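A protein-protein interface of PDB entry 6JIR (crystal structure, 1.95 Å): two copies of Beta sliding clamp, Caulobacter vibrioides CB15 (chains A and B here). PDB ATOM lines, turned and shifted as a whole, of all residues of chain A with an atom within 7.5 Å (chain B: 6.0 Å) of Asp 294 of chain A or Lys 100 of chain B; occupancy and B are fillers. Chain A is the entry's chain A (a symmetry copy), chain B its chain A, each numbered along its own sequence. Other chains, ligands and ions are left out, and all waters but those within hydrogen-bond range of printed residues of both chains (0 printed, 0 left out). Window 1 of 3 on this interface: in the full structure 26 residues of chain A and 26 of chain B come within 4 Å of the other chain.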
ATOM      1  N   LEU A 288      -3.773   0.762  24.935  1.00  0.00           N
ATOM      2  CA  LEU A 288      -3.124  -0.005  23.863  1.00  0.00           C
ATOM      3  C   LEU A 288      -3.308  -1.492  24.033  1.00  0.00           C
ATOM      4  O   LEU A 288      -3.667  -2.201  23.094  1.00  0.00           O
ATOM      5  CB  LEU A 288      -1.618   0.320  23.760  1.00  0.00           C
ATOM      6  CG  LEU A 288      -1.198   1.466  22.827  1.00  0.00           C
ATOM      7  CD1 LEU A 288      -1.381   1.058  21.358  1.00  0.00           C
ATOM      8  CD2 LEU A 288      -1.936   2.783  23.084  1.00  0.00           C
ATOM      9  N   PHE A 289      -3.062  -1.969  25.247  1.00  0.00           N
ATOM     10  CA  PHE A 289      -3.168  -3.382  25.537  1.00  0.00           C
ATOM     11  C   PHE A 289      -4.600  -3.876  25.396  1.00  0.00           C
ATOM     12  O   PHE A 289      -4.842  -4.924  24.791  1.00  0.00           O
ATOM     13  CB  PHE A 289      -2.665  -3.649  26.946  1.00  0.00           C
ATOM     14  CG  PHE A 289      -2.720  -5.066  27.352  1.00  0.00           C
ATOM     15  CD1 PHE A 289      -1.811  -5.984  26.839  1.00  0.00           C
ATOM     16  CD2 PHE A 289      -3.653  -5.491  28.271  1.00  0.00           C
ATOM     17  CE1 PHE A 289      -1.834  -7.304  27.258  1.00  0.00           C
ATOM     18  CE2 PHE A 289      -3.702  -6.815  28.680  1.00  0.00           C
ATOM     19  CZ  PHE A 289      -2.796  -7.727  28.167  1.00  0.00           C
ATOM     20  N   ALA A 290      -5.543  -3.150  25.980  1.00  0.00           N
ATOM     21  CA  ALA A 290      -6.959  -3.559  25.901  1.00  0.00           C
ATOM     22  C   ALA A 290      -7.432  -3.597  24.407  1.00  0.00           C
ATOM     23  O   ALA A 290      -8.211  -4.471  24.002  1.00  0.00           O
ATOM     24  CB  ALA A 290      -7.800  -2.594  26.691  1.00  0.00           C
ATOM     25  N   LYS A 291      -6.978  -2.633  23.632  1.00  0.00           N
ATOM     26  CA  LYS A 291      -7.304  -2.578  22.198  1.00  0.00           C
ATOM     27  C   LYS A 291      -6.725  -3.777  21.463  1.00  0.00           C
ATOM     28  O   LYS A 291      -7.419  -4.413  20.662  1.00  0.00           O
ATOM     29  CB  LYS A 291      -6.831  -1.267  21.607  1.00  0.00           C
ATOM     30  CG  LYS A 291      -7.781  -0.139  21.967  1.00  0.00           C
ATOM     31  CD  LYS A 291      -7.363   1.201  21.394  1.00  0.00           C
ATOM     32  CE  LYS A 291      -8.428   2.242  21.746  1.00  0.00           C
ATOM     33  NZ  LYS A 291      -7.881   3.613  21.564  1.00  0.00           N
ATOM     34  N   ALA A 292      -5.488  -4.147  21.812  1.00  0.00           N
ATOM     35  CA  ALA A 292      -4.855  -5.362  21.267  1.00  0.00           C
ATOM     36  C   ALA A 292      -5.617  -6.637  21.575  1.00  0.00           C
ATOM     37  O   ALA A 292      -5.897  -7.458  20.666  1.00  0.00           O
ATOM     38  CB  ALA A 292      -3.427  -5.495  21.779  1.00  0.00           C
ATOM     39  N   VAL A 293      -5.959  -6.812  22.845  1.00  0.00           N
ATOM     40  CA  VAL A 293      -6.719  -7.983  23.311  1.00  0.00           C
ATOM     41  C   VAL A 293      -8.064  -8.081  22.574  1.00  0.00           C
ATOM     42  O   VAL A 293      -8.454  -9.147  22.143  1.00  0.00           O
ATOM     43  CB  VAL A 293      -6.981  -7.926  24.831  1.00  0.00           C
ATOM     44  CG1 VAL A 293      -7.945  -8.992  25.284  1.00  0.00           C
ATOM     45  CG2 VAL A 293      -5.671  -8.061  25.598  1.00  0.00           C
ATOM     46  N   ASP A 294      -8.770  -6.957  22.502  1.00  0.00           N
ATOM     47  CA  ASP A 294     -10.087  -6.888  21.865  1.00  0.00           C
ATOM     48  C   ASP A 294      -9.953  -7.190  20.362  1.00  0.00           C
ATOM     49  O   ASP A 294     -10.732  -7.957  19.789  1.00  0.00           O
ATOM     50  CB  ASP A 294     -10.692  -5.511  22.144  1.00  0.00           C
ATOM     51  CG  ASP A 294     -12.093  -5.347  21.575  1.00  0.00           C
ATOM     52  OD1 ASP A 294     -12.988  -6.115  21.922  1.00  0.00           O
ATOM     53  OD2 ASP A 294     -12.275  -4.431  20.774  1.00  0.00           O
ATOM     54  N   ARG A 295      -8.905  -6.668  19.770  1.00  0.00           N
ATOM     55  CA  ARG A 295      -8.600  -6.904  18.390  1.00  0.00           C
ATOM     56  C   ARG A 295      -8.368  -8.378  18.160  1.00  0.00           C
ATOM     57  O   ARG A 295      -9.032  -8.981  17.390  1.00  0.00           O
ATOM     58  CB  ARG A 295      -7.355  -6.138  18.011  1.00  0.00           C
ATOM     59  CG  ARG A 295      -7.187  -5.784  16.581  1.00  0.00           C
ATOM     60  CD  ARG A 295      -5.987  -4.879  16.427  1.00  0.00           C
ATOM     61  NE  ARG A 295      -6.265  -3.483  16.736  1.00  0.00           N
ATOM     62  CZ  ARG A 295      -5.593  -2.749  17.597  1.00  0.00           C
ATOM     63  NH1 ARG A 295      -4.618  -3.245  18.286  1.00  0.00           N
ATOM     64  NH2 ARG A 295      -5.914  -1.505  17.767  1.00  0.00           N
ATOM     65  N   VAL A 296      -7.422  -8.967  18.858  1.00  0.00           N
ATOM     66  CA  VAL A 296      -7.158 -10.403  18.629  1.00  0.00           C
ATOM     67  C   VAL A 296      -8.325 -11.307  18.997  1.00  0.00           C
ATOM     68  O   VAL A 296      -8.497 -12.358  18.364  1.00  0.00           O
ATOM     69  CB  VAL A 296      -5.850 -10.952  19.267  1.00  0.00           C
ATOM     70  CG1 VAL A 296      -4.622 -10.344  18.585  1.00  0.00           C
ATOM     71  CG2 VAL A 296      -5.823 -10.809  20.797  1.00  0.00           C
ATOM     72  N   ALA A 297      -9.119 -10.931  20.016  1.00  0.00           N
ATOM     73  CA  ALA A 297     -10.282 -11.745  20.394  1.00  0.00           C
ATOM     74  C   ALA A 297     -11.320 -11.833  19.271  1.00  0.00           C
ATOM     75  O   ALA A 297     -12.115 -12.782  19.236  1.00  0.00           O
ATOM     76  CB  ALA A 297     -10.940 -11.216  21.670  1.00  0.00           C
ATOM     77  N   THR A 298     -11.305 -10.838  18.381  1.00  0.00           N
ATOM     78  CA  THR A 298     -12.273 -10.691  17.298  1.00  0.00           C
ATOM     79  C   THR A 298     -12.144 -11.809  16.262  1.00  0.00           C
ATOM     80  O   THR A 298     -13.019 -11.966  15.444  1.00  0.00           O
ATOM     81  CB  THR A 298     -12.149  -9.306  16.651  1.00  0.00           C
ATOM     82  OG1 THR A 298     -12.427  -8.285  17.635  1.00  0.00           O
ATOM     83  CG2 THR A 298     -13.147  -9.102  15.514  1.00  0.00           C
ATOM     84  N   ILE A 299     -11.063 -12.591  16.304  1.00  0.00           N
ATOM     85  CA  ILE A 299     -10.969 -13.835  15.530  1.00  0.00           C
ATOM     86  C   ILE A 299     -12.085 -14.824  15.885  1.00  0.00           C
ATOM     87  O   ILE A 299     -12.396 -15.684  15.090  1.00  0.00           O
ATOM     88  CB  ILE A 299      -9.575 -14.518  15.684  1.00  0.00           C
ATOM     89  CG1 ILE A 299      -9.323 -15.605  14.619  1.00  0.00           C
ATOM     90  CG2 ILE A 299      -9.377 -15.095  17.070  1.00  0.00           C
ATOM     91  CD1 ILE A 299      -9.021 -15.055  13.244  1.00  0.00           C
ATOM     92  N   SER A 300     -12.665 -14.707  17.072  1.00  0.00           N
ATOM     93  CA  SER A 300     -13.628 -15.686  17.584  1.00  0.00           C
ATOM     94  C   SER A 300     -14.936 -15.007  17.986  1.00  0.00           C
ATOM     95  O   SER A 300     -14.924 -13.899  18.508  1.00  0.00           O
ATOM     96  CB  SER A 300     -13.023 -16.448  18.770  1.00  0.00           C
ATOM     97  OG  SER A 300     -13.954 -17.365  19.303  1.00  0.00           O
ATOM     98  N   ARG A 305     -14.046 -16.773  25.209  1.00  0.00           N
ATOM     99  CA  ARG A 305     -12.843 -16.665  24.385  1.00  0.00           C
ATOM    100  C   ARG A 305     -11.621 -16.523  25.302  1.00  0.00           C
ATOM    101  O   ARG A 305     -11.629 -15.674  26.182  1.00  0.00           O
ATOM    102  CB  ARG A 305     -12.926 -15.446  23.447  1.00  0.00           C
ATOM    103  CG  ARG A 305     -14.169 -15.412  22.559  1.00  0.00           C
ATOM    104  CD  ARG A 305     -14.251 -14.180  21.668  1.00  0.00           C
ATOM    105  NE  ARG A 305     -14.404 -12.938  22.412  1.00  0.00           N
ATOM    106  CZ  ARG A 305     -14.594 -11.734  21.875  1.00  0.00           C
ATOM    107  NH1 ARG A 305     -14.645 -11.567  20.545  1.00  0.00           N
ATOM    108  NH2 ARG A 305     -14.728 -10.678  22.677  1.00  0.00           N
ATOM    109  N   VAL A 307      -7.385 -15.906  25.731  1.00  0.00           N
ATOM    110  CA  VAL A 307      -6.227 -15.285  25.098  1.00  0.00           C
ATOM    111  C   VAL A 307      -4.948 -15.755  25.823  1.00  0.00           C
ATOM    112  O   VAL A 307      -4.937 -15.886  27.051  1.00  0.00           O
ATOM    113  CB  VAL A 307      -6.328 -13.753  25.054  1.00  0.00           C
ATOM    114  CG1 VAL A 307      -6.438 -13.141  26.448  1.00  0.00           C
ATOM    115  CG2 VAL A 307      -5.163 -13.135  24.286  1.00  0.00           C
ATOM    116  N   LEU A 318       0.285 -11.636  22.234  1.00  0.00           N
ATOM    117  CA  LEU A 318      -1.079 -12.091  22.460  1.00  0.00           C
ATOM    118  C   LEU A 318      -1.527 -12.987  21.307  1.00  0.00           C
ATOM    119  O   LEU A 318      -1.391 -12.594  20.131  1.00  0.00           O
ATOM    120  CB  LEU A 318      -2.017 -10.907  22.485  1.00  0.00           C
ATOM    121  CG  LEU A 318      -1.799  -9.875  23.577  1.00  0.00           C
ATOM    122  CD1 LEU A 318      -2.497  -8.573  23.215  1.00  0.00           C
ATOM    123  CD2 LEU A 318      -2.317 -10.456  24.850  1.00  0.00           C
ATOM    124  N   VAL A 320      -4.932 -15.446  20.065  1.00  0.00           N
ATOM    125  CA  VAL A 320      -6.269 -16.042  20.185  1.00  0.00           C
ATOM    126  C   VAL A 320      -6.481 -16.957  18.972  1.00  0.00           C
ATOM    127  O   VAL A 320      -6.032 -16.656  17.860  1.00  0.00           O
ATOM    128  CB  VAL A 320      -7.394 -14.975  20.253  1.00  0.00           C
ATOM    129  CG1 VAL A 320      -8.793 -15.605  20.344  1.00  0.00           C
ATOM    130  CG2 VAL A 320      -7.195 -14.032  21.455  1.00  0.00           C
ATOM    131  N   GLU A 330      -0.845 -10.512  18.135  1.00  0.00           N
ATOM    132  CA  GLU A 330      -0.377  -9.147  18.240  1.00  0.00           C
ATOM    133  C   GLU A 330       0.701  -8.990  19.328  1.00  0.00           C
ATOM    134  O   GLU A 330       0.595  -9.552  20.418  1.00  0.00           O
ATOM    135  CB  GLU A 330      -1.545  -8.179  18.468  1.00  0.00           C
ATOM    136  CG  GLU A 330      -1.133  -6.692  18.572  1.00  0.00           C
ATOM    137  CD  GLU A 330      -2.258  -5.707  18.302  1.00  0.00           C
ATOM    138  OE1 GLU A 330      -3.389  -6.146  18.040  1.00  0.00           O
ATOM    139  OE2 GLU A 330      -2.027  -4.475  18.328  1.00  0.00           O
ATOM    140  N   ALA A 347     -10.627 -13.660  27.863  1.00  0.00           N
ATOM    141  CA  ALA A 347     -10.443 -12.317  27.295  1.00  0.00           C
ATOM    142  C   ALA A 347     -11.412 -11.275  27.882  1.00  0.00           C
ATOM    143  O   ALA A 347     -11.003 -10.129  28.107  1.00  0.00           O
ATOM    144  CB  ALA A 347     -10.558 -12.339  25.770  1.00  0.00           C
ATOM    145  N   ARG A 348     -12.671 -11.659  28.109  1.00  0.00           N
ATOM    146  CA  ARG A 348     -13.668 -10.749  28.684  1.00  0.00           C
ATOM    147  C   ARG A 348     -13.287 -10.350  30.118  1.00  0.00           C
ATOM    148  O   ARG A 348     -13.428  -9.194  30.465  1.00  0.00           O
ATOM    149  CB  ARG A 348     -15.094 -11.341  28.676  1.00  0.00           C
ATOM    150  CG  ARG A 348     -16.188 -10.433  29.293  1.00  0.00           C
ATOM    151  CD  ARG A 348     -16.220  -8.992  28.747  1.00  0.00           C
ATOM    152  NE  ARG A 348     -16.254  -8.992  27.281  1.00  0.00           N
ATOM    153  CZ  ARG A 348     -15.922  -7.979  26.464  1.00  0.00           C
ATOM    154  NH1 ARG A 348     -15.993  -8.163  25.144  1.00  0.00           N
ATOM    155  NH2 ARG A 348     -15.516  -6.801  26.921  1.00  0.00           N
ATOM    156  N   LEU A 351     -10.502  -7.881  29.811  1.00  0.00           N
ATOM    157  CA  LEU A 351     -11.016  -6.615  29.319  1.00  0.00           C
ATOM    158  C   LEU A 351     -11.842  -5.836  30.354  1.00  0.00           C
ATOM    159  O   LEU A 351     -11.775  -4.604  30.364  1.00  0.00           O
ATOM    160  CB  LEU A 351     -11.837  -6.814  28.024  1.00  0.00           C
ATOM    161  CG  LEU A 351     -11.009  -7.161  26.783  1.00  0.00           C
ATOM    162  CD1 LEU A 351     -11.943  -7.580  25.632  1.00  0.00           C
ATOM    163  CD2 LEU A 351     -10.104  -6.033  26.375  1.00  0.00           C
ATOM    164  N   ARG B  27      -7.454   0.853   5.120  1.00  0.00           N
ATOM    165  CA  ARG B  27      -8.491   0.306   5.999  1.00  0.00           C
ATOM    166  C   ARG B  27      -9.884   0.834   5.667  1.00  0.00           C
ATOM    167  O   ARG B  27     -10.835   0.062   5.654  1.00  0.00           O
ATOM    168  CB  ARG B  27      -8.206   0.562   7.488  1.00  0.00           C
ATOM    169  CG  ARG B  27      -9.357   0.137   8.401  1.00  0.00           C
ATOM    170  CD  ARG B  27      -9.108   0.387   9.869  1.00  0.00           C
ATOM    171  NE  ARG B  27     -10.334   0.133  10.634  1.00  0.00           N
ATOM    172  CZ  ARG B  27     -11.345   0.995  10.798  1.00  0.00           C
ATOM    173  NH1 ARG B  27     -11.300   2.212  10.286  1.00  0.00           N
ATOM    174  NH2 ARG B  27     -12.400   0.639  11.512  1.00  0.00           N
ATOM    175  N   TYR B  95     -14.833  -9.075   8.076  1.00  0.00           N
ATOM    176  CA  TYR B  95     -15.421  -7.747   8.313  1.00  0.00           C
ATOM    177  C   TYR B  95     -15.150  -7.298   9.764  1.00  0.00           C
ATOM    178  O   TYR B  95     -14.672  -6.169   9.976  1.00  0.00           O
ATOM    179  CB  TYR B  95     -16.913  -7.799   8.041  1.00  0.00           C
ATOM    180  CG  TYR B  95     -17.662  -6.534   8.361  1.00  0.00           C
ATOM    181  CD1 TYR B  95     -17.351  -5.360   7.738  1.00  0.00           C
ATOM    182  CD2 TYR B  95     -18.716  -6.548   9.274  1.00  0.00           C
ATOM    183  CE1 TYR B  95     -18.047  -4.195   8.011  1.00  0.00           C
ATOM    184  CE2 TYR B  95     -19.429  -5.389   9.564  1.00  0.00           C
ATOM    185  CZ  TYR B  95     -19.076  -4.217   8.932  1.00  0.00           C
ATOM    186  OH  TYR B  95     -19.763  -3.071   9.217  1.00  0.00           O
ATOM    187  N   GLU B  96     -15.415  -8.187  10.727  1.00  0.00           N
ATOM    188  CA  GLU B  96     -15.265  -7.867  12.153  1.00  0.00           C
ATOM    189  C   GLU B  96     -13.817  -7.550  12.487  1.00  0.00           C
ATOM    190  O   GLU B  96     -13.532  -6.594  13.201  1.00  0.00           O
ATOM    191  CB  GLU B  96     -15.838  -8.962  13.068  1.00  0.00           C
ATOM    192  CG  GLU B  96     -17.361  -9.169  12.973  1.00  0.00           C
ATOM    193  CD  GLU B  96     -18.190  -7.944  13.392  1.00  0.00           C
ATOM    194  OE1 GLU B  96     -19.355  -7.806  12.939  1.00  0.00           O
ATOM    195  OE2 GLU B  96     -17.674  -7.074  14.138  1.00  0.00           O
ATOM    196  N   ILE B  97     -12.883  -8.326  11.943  1.00  0.00           N
ATOM    197  CA  ILE B  97     -11.463  -8.041  12.064  1.00  0.00           C
ATOM    198  C   ILE B  97     -11.109  -6.614  11.604  1.00  0.00           C
ATOM    199  O   ILE B  97     -10.535  -5.810  12.365  1.00  0.00           O
ATOM    200  CB  ILE B  97     -10.593  -9.081  11.308  1.00  0.00           C
ATOM    201  CG1 ILE B  97     -10.671 -10.442  12.009  1.00  0.00           C
ATOM    202  CG2 ILE B  97      -9.133  -8.643  11.262  1.00  0.00           C
ATOM    203  CD1 ILE B  97     -10.063 -11.593  11.180  1.00  0.00           C
ATOM    204  N   VAL B  98     -11.495  -6.298  10.384  1.00  0.00           N
ATOM    205  CA  VAL B  98     -11.173  -5.026   9.746  1.00  0.00           C
ATOM    206  C   VAL B  98     -11.777  -3.863  10.553  1.00  0.00           C
ATOM    207  O   VAL B  98     -11.126  -2.838  10.728  1.00  0.00           O
ATOM    208  CB  VAL B  98     -11.591  -5.042   8.246  1.00  0.00           C
ATOM    209  CG1 VAL B  98     -11.386  -3.710   7.562  1.00  0.00           C
ATOM    210  CG2 VAL B  98     -10.752  -6.069   7.484  1.00  0.00           C
ATOM    211  N   ARG B  99     -12.989  -4.027  11.067  1.00  0.00           N
ATOM    212  CA  ARG B  99     -13.578  -3.051  11.985  1.00  0.00           C
ATOM    213  C   ARG B  99     -12.676  -2.700  13.172  1.00  0.00           C
ATOM    214  O   ARG B  99     -12.606  -1.535  13.574  1.00  0.00           O
ATOM    215  CB  ARG B  99     -14.903  -3.550  12.549  1.00  0.00           C
ATOM    216  CG  ARG B  99     -16.064  -3.523  11.585  1.00  0.00           C
ATOM    217  CD  ARG B  99     -17.296  -4.091  12.255  1.00  0.00           C
ATOM    218  NE  ARG B  99     -17.842  -3.187  13.264  1.00  0.00           N
ATOM    219  CZ  ARG B  99     -18.819  -3.488  14.123  1.00  0.00           C
ATOM    220  NH1 ARG B  99     -19.389  -4.696  14.138  1.00  0.00           N
ATOM    221  NH2 ARG B  99     -19.231  -2.558  14.990  1.00  0.00           N
ATOM    222  N   LYS B 100     -11.998  -3.700  13.730  1.00  0.00           N
ATOM    223  CA  LYS B 100     -11.129  -3.495  14.888  1.00  0.00           C
ATOM    224  C   LYS B 100      -9.747  -2.969  14.562  1.00  0.00           C
ATOM    225  O   LYS B 100      -9.010  -2.633  15.468  1.00  0.00           O
ATOM    226  CB  LYS B 100     -10.970  -4.777  15.695  1.00  0.00           C
ATOM    227  CG  LYS B 100     -12.235  -5.340  16.260  1.00  0.00           C
ATOM    228  CD  LYS B 100     -12.878  -4.399  17.245  1.00  0.00           C
ATOM    229  CE  LYS B 100     -13.915  -5.113  18.101  1.00  0.00           C
ATOM    230  NZ  LYS B 100     -14.394  -4.162  19.135  1.00  0.00           N
ATOM    231  N   LEU B 101      -9.342  -2.956  13.304  1.00  0.00           N
ATOM    232  CA  LEU B 101      -7.984  -2.522  12.978  1.00  0.00           C
ATOM    233  C   LEU B 101      -7.884  -1.006  13.226  1.00  0.00           C
ATOM    234  O   LEU B 101      -8.891  -0.311  13.090  1.00  0.00           O
ATOM    235  CB  LEU B 101      -7.608  -2.875  11.547  1.00  0.00           C
ATOM    236  CG  LEU B 101      -7.569  -4.377  11.258  1.00  0.00           C
ATOM    237  CD1 LEU B 101      -7.318  -4.625   9.772  1.00  0.00           C
ATOM    238  CD2 LEU B 101      -6.532  -5.113  12.118  1.00  0.00           C
ATOM    239  N   PRO B 102      -6.684  -0.504  13.598  1.00  0.00           N
ATOM    240  CA  PRO B 102      -6.584   0.919  13.906  1.00  0.00           C
ATOM    241  C   PRO B 102      -6.971   1.812  12.730  1.00  0.00           C
ATOM    242  O   PRO B 102      -6.648   1.521  11.578  1.00  0.00           O
ATOM    243  CB  PRO B 102      -5.104   1.113  14.266  1.00  0.00           C
ATOM    244  CG  PRO B 102      -4.600  -0.231  14.633  1.00  0.00           C
ATOM    245  CD  PRO B 102      -5.384  -1.184  13.758  1.00  0.00           C
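The side-chain carboxylate (OD2) of Asp 294 of chain A is in salt-bridge range of the side-chain amino group (NZ) of Lys 100 of chain B, at 2.7 Å. The backbone carbonyl oxygen (O) of Lys 100 of chain B lies within hydrogen-bond range of the guanidinium group (NE) of Arg 295 of chain A (3.1 Å).
Of chain B, only Lys 100 (2.7 Å) comes within 4 Å of Asp 294 of chain A. Lys 100 of chain B touches just these residues of chain A: Asp 294 (2.7 Å), Arg 295 (3.1 Å) and Thr 298 (3.3 Å). Of the printed residues of chain B, Thr 298 of chain A touches Glu 96 (3.4 Å), Ile 97 (3.7 Å) and Lys 100 (3.3 Å). Of the printed residues of chain A, Ile 97 of chain B touches Thr 298 (3.7 Å). Printed residues of chain A within 4 Å of Pro 102 of chain B: Arg 295. Ile 299 of chain A touches none of the printed residues of chain B. The nearest printed residue of chain A that does not touch Glu 96 of chain B is Arg 295 of chain A (6.6 Å).
No position is printed for both chains. Of the 6 pairs that touch across the chains among the printed residues, none has its exchanged pair printed and touching as well.
Printed residues of chain B that touch a printed residue of chain A: Glu 96, Ile 97, Lys 100 and Pro 102. Among the printed residues, 6 pairs touch across the chains. Among the printed residues, Asp or Glu carboxylates within 4 Å of a Lys or Arg side-chain nitrogen of the other chain: Asp 294 of chain A with Lys 100 of chain B (2.7 Å).
Arg 295 of chain A touches Pro 102 of chain B (NH2 to CG, 3.6 Å). Glu 96 of chain B touches Thr 298 of chain A (O to CG2, 3.4 Å). CG2 of Thr 298 of chain A touches N of Ile 97 of chain B (3.7 Å). Lys 100 of chain B touches Thr 298 of chain A.
OE2 of Glu 96 of chain B lies within salt-bridge range of NH1 of Arg 99 of chain B (2.9 Å). OG1 of Thr 298 of chain A sits at hydrogen-bond distance from O of Asp 294 of chain A (2.8 Å). O of Arg 295 of chain A sits close to OG1 of Thr 298 of chain A (3.5 Å). NH1 of Arg 295 of chain A lies within salt-bridge range of OE2 of Glu 330 of chain A (2.9 Å).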
